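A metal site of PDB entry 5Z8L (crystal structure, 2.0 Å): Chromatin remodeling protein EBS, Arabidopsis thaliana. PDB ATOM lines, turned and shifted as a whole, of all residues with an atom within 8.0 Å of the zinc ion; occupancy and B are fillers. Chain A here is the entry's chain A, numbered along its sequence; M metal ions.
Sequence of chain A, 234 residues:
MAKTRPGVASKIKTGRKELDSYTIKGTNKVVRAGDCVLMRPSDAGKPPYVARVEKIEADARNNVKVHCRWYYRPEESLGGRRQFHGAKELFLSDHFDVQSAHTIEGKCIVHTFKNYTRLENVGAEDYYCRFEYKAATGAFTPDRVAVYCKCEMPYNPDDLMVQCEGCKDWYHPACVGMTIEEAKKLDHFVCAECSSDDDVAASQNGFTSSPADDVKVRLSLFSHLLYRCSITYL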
ATOM      1  N   GLN A 163      12.531 -21.213   0.665  1.00  0.00           N
ATOM      2  CA  GLN A 163      12.731 -21.494  -0.750  1.00  0.00           C
ATOM      3  C   GLN A 163      13.043 -22.970  -0.986  1.00  0.00           C
ATOM      4  O   GLN A 163      13.851 -23.573  -0.281  1.00  0.00           O
ATOM      5  CB  GLN A 163      13.858 -20.627  -1.312  1.00  0.00           C
ATOM      6  CG  GLN A 163      14.149 -20.876  -2.788  1.00  0.00           C
ATOM      7  CD  GLN A 163      15.189 -19.929  -3.344  1.00  0.00           C
ATOM      8  OE1 GLN A 163      16.303 -19.838  -2.836  1.00  0.00           O
ATOM      9  NE2 GLN A 163      14.825 -19.207  -4.400  1.00  0.00           N
ATOM     10  N   CYS A 164      12.390 -23.549  -1.988  1.00  0.00           N
ATOM     11  CA  CYS A 164      12.699 -24.897  -2.415  1.00  0.00           C
ATOM     12  C   CYS A 164      14.026 -24.942  -3.149  1.00  0.00           C
ATOM     13  O   CYS A 164      14.340 -24.060  -3.948  1.00  0.00           O
ATOM     14  CB  CYS A 164      11.598 -25.457  -3.307  1.00  0.00           C
ATOM     15  SG  CYS A 164      12.028 -27.018  -4.113  1.00  0.00           S
ATOM     16  N   GLU A 165      14.807 -25.998  -2.891  1.00  0.00           N
ATOM     17  CA  GLU A 165      16.095 -26.172  -3.549  1.00  0.00           C
ATOM     18  C   GLU A 165      15.933 -26.717  -4.965  1.00  0.00           C
ATOM     19  O   GLU A 165      16.903 -27.083  -5.609  1.00  0.00           O
ATOM     20  CB  GLU A 165      16.988 -27.085  -2.719  1.00  0.00           C
ATOM     21  CG  GLU A 165      18.252 -26.403  -2.191  1.00  0.00           C
ATOM     22  CD  GLU A 165      18.919 -27.214  -1.097  1.00  0.00           C
ATOM     23  OE1 GLU A 165      18.210 -27.696  -0.197  1.00  0.00           O
ATOM     24  OE2 GLU A 165      20.165 -27.351  -1.140  1.00  0.00           O
ATOM     25  N   GLY A 166      14.688 -26.785  -5.430  1.00  0.00           N
ATOM     26  CA  GLY A 166      14.395 -27.252  -6.768  1.00  0.00           C
ATOM     27  C   GLY A 166      13.724 -26.188  -7.626  1.00  0.00           C
ATOM     28  O   GLY A 166      14.226 -25.842  -8.696  1.00  0.00           O
ATOM     29  N   CYS A 167      12.592 -25.671  -7.148  1.00  0.00           N
ATOM     30  CA  CYS A 167      11.837 -24.683  -7.919  1.00  0.00           C
ATOM     31  C   CYS A 167      12.489 -23.309  -7.859  1.00  0.00           C
ATOM     32  O   CYS A 167      12.353 -22.518  -8.789  1.00  0.00           O
ATOM     33  CB  CYS A 167      10.400 -24.545  -7.384  1.00  0.00           C
ATOM     34  SG  CYS A 167       9.727 -25.973  -6.529  1.00  0.00           S
ATOM     35  N   LYS A 168      13.156 -23.044  -6.731  1.00  0.00           N
ATOM     36  CA  LYS A 168      13.560 -21.698  -6.314  1.00  0.00           C
ATOM     37  C   LYS A 168      12.317 -20.880  -5.975  1.00  0.00           C
ATOM     38  O   LYS A 168      12.405 -19.681  -5.677  1.00  0.00           O
ATOM     39  CB  LYS A 168      14.408 -20.983  -7.371  1.00  0.00           C
ATOM     40  CG  LYS A 168      15.574 -21.807  -7.897  1.00  0.00           C
ATOM     41  CD  LYS A 168      16.358 -22.458  -6.768  1.00  0.00           C
ATOM     42  CE  LYS A 168      17.171 -23.640  -7.265  1.00  0.00           C
ATOM     43  NZ  LYS A 168      17.762 -24.430  -6.153  1.00  0.00           N
ATOM     44  N   ASP A 169      11.156 -21.528  -6.013  1.00  0.00           N
ATOM     45  CA  ASP A 169       9.901 -20.936  -5.601  1.00  0.00           C
ATOM     46  C   ASP A 169       9.883 -20.822  -4.081  1.00  0.00           C
ATOM     47  O   ASP A 169      10.541 -21.619  -3.391  1.00  0.00           O
ATOM     48  CB  ASP A 169       8.722 -21.785  -6.099  1.00  0.00           C
ATOM     49  CG  ASP A 169       7.376 -21.095  -5.941  1.00  0.00           C
ATOM     50  OD1 ASP A 169       7.359 -19.872  -5.688  1.00  0.00           O
ATOM     51  OD2 ASP A 169       6.346 -21.784  -6.074  1.00  0.00           O
ATOM     52  N   TYR A 171       7.754 -20.560  -0.336  1.00  0.00           N
ATOM     53  CA  TYR A 171       6.547 -21.114   0.245  1.00  0.00           C
ATOM     54  C   TYR A 171       6.295 -20.609   1.656  1.00  0.00           C
ATOM     55  O   TYR A 171       7.210 -20.525   2.474  1.00  0.00           O
ATOM     56  CB  TYR A 171       6.620 -22.646   0.272  1.00  0.00           C
ATOM     57  CG  TYR A 171       6.554 -23.296  -1.085  1.00  0.00           C
ATOM     58  CD1 TYR A 171       7.715 -23.545  -1.801  1.00  0.00           C
ATOM     59  CD2 TYR A 171       5.341 -23.668  -1.642  1.00  0.00           C
ATOM     60  CE1 TYR A 171       7.668 -24.146  -3.050  1.00  0.00           C
ATOM     61  CE2 TYR A 171       5.282 -24.262  -2.885  1.00  0.00           C
ATOM     62  CZ  TYR A 171       6.440 -24.498  -3.586  1.00  0.00           C
ATOM     63  OH  TYR A 171       6.380 -25.100  -4.822  1.00  0.00           O
ATOM     64  N   PHE A 189      15.375 -27.651   2.395  1.00  0.00           N
ATOM     65  CA  PHE A 189      13.984 -27.784   2.021  1.00  0.00           C
ATOM     66  C   PHE A 189      13.791 -28.071   0.536  1.00  0.00           C
ATOM     67  O   PHE A 189      14.137 -27.247  -0.313  1.00  0.00           O
ATOM     68  CB  PHE A 189      13.197 -26.535   2.413  1.00  0.00           C
ATOM     69  CG  PHE A 189      11.787 -26.549   1.945  1.00  0.00           C
ATOM     70  CD1 PHE A 189      10.885 -27.424   2.511  1.00  0.00           C
ATOM     71  CD2 PHE A 189      11.377 -25.699   0.943  1.00  0.00           C
ATOM     72  CE1 PHE A 189       9.581 -27.448   2.075  1.00  0.00           C
ATOM     73  CE2 PHE A 189      10.072 -25.709   0.509  1.00  0.00           C
ATOM     74  CZ  PHE A 189       9.168 -26.591   1.080  1.00  0.00           C
ATOM     75  N   VAL A 190      13.236 -29.227   0.216  1.00  0.00           N
ATOM     76  CA  VAL A 190      12.765 -29.520  -1.139  1.00  0.00           C
ATOM     77  C   VAL A 190      11.289 -29.744  -1.132  1.00  0.00           C
ATOM     78  O   VAL A 190      10.802 -30.553  -0.408  1.00  0.00           O
ATOM     79  CB  VAL A 190      13.421 -30.746  -1.769  1.00  0.00           C
ATOM     80  CG1 VAL A 190      12.911 -30.960  -3.160  1.00  0.00           C
ATOM     81  CG2 VAL A 190      14.917 -30.574  -1.820  1.00  0.00           C
ATOM     82  N   CYS A 191      10.596 -28.997  -1.948  1.00  0.00           N
ATOM     83  CA  CYS A 191       9.153 -29.004  -1.960  1.00  0.00           C
ATOM     84  C   CYS A 191       8.535 -30.153  -2.715  1.00  0.00           C
ATOM     85  O   CYS A 191       9.160 -30.772  -3.515  1.00  0.00           O
ATOM     86  CB  CYS A 191       8.621 -27.660  -2.437  1.00  0.00           C
ATOM     87  SG  CYS A 191       7.805 -27.525  -4.027  1.00  0.00           S
ATOM     88  N   ALA A 192       7.289 -30.443  -2.385  1.00  0.00           N
ATOM     89  CA  ALA A 192       6.523 -31.552  -2.954  1.00  0.00           C
ATOM     90  C   ALA A 192       6.176 -31.437  -4.433  1.00  0.00           C
ATOM     91  O   ALA A 192       5.882 -32.397  -5.064  1.00  0.00           O
ATOM     92  CB  ALA A 192       5.287 -31.806  -2.128  1.00  0.00           C
ATOM     93  N   GLU A 193       6.136 -30.215  -4.948  1.00  0.00           N
ATOM     94  CA  GLU A 193       6.036 -30.004  -6.361  1.00  0.00           C
ATOM     95  C   GLU A 193       7.289 -30.572  -6.994  1.00  0.00           C
ATOM     96  O   GLU A 193       7.292 -30.913  -8.146  1.00  0.00           O
ATOM     97  CB  GLU A 193       5.823 -28.520  -6.726  1.00  0.00           C
ATOM     98  CG  GLU A 193       4.383 -28.160  -7.081  1.00  0.00           C
ATOM     99  CD  GLU A 193       4.110 -26.656  -7.290  1.00  0.00           C
ATOM    100  OE1 GLU A 193       4.813 -26.012  -8.090  1.00  0.00           O
ATOM    101  OE2 GLU A 193       3.157 -26.123  -6.678  1.00  0.00           O
ATOM    102  N   CYS A 194       8.363 -30.594  -6.235  1.00  0.00           N
ATOM    103  CA  CYS A 194       9.628 -31.095  -6.724  1.00  0.00           C
ATOM    104  C   CYS A 194       9.862 -32.587  -6.413  1.00  0.00           C
ATOM    105  O   CYS A 194       9.891 -33.024  -5.277  1.00  0.00           O
ATOM    106  CB  CYS A 194      10.756 -30.198  -6.238  1.00  0.00           C
ATOM    107  SG  CYS A 194      11.187 -28.865  -7.360  1.00  0.00           S
HETATM  108 ZN    ZN M   1       9.816 -27.712  -5.127  1.00  0.00          ZN
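The backbone NH of Gly 166 lies close to the side-chain sulfur of Cys 164 (3.0 Å).
SG of Cys 191 lies close to N of Glu 193, at 3.3 Å.
N of Cys 164 lies within hydrogen-bond range of O of Asp 169 (3.0 Å).
The side-chain sulfur of Cys 191 lies close to the side-chain hydroxyl of Tyr 171 (2.9 Å).
N of Cys 167 lies within hydrogen-bond range of SG of Cys 194, at 3.5 Å.
The nearest printed residue that does not touch the zinc ion is Glu 193 (4.2 Å).
The zinc ion is bound by SG of Cys 167 (2.2 Å), SG of Cys 191 (2.3 Å) and SG of Cys 164 (2.5 Å).
The zinc ion has three donor atoms within binding distance.
Slightly farther from the zinc ion lies SG of Cys 194 (2.9 Å).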
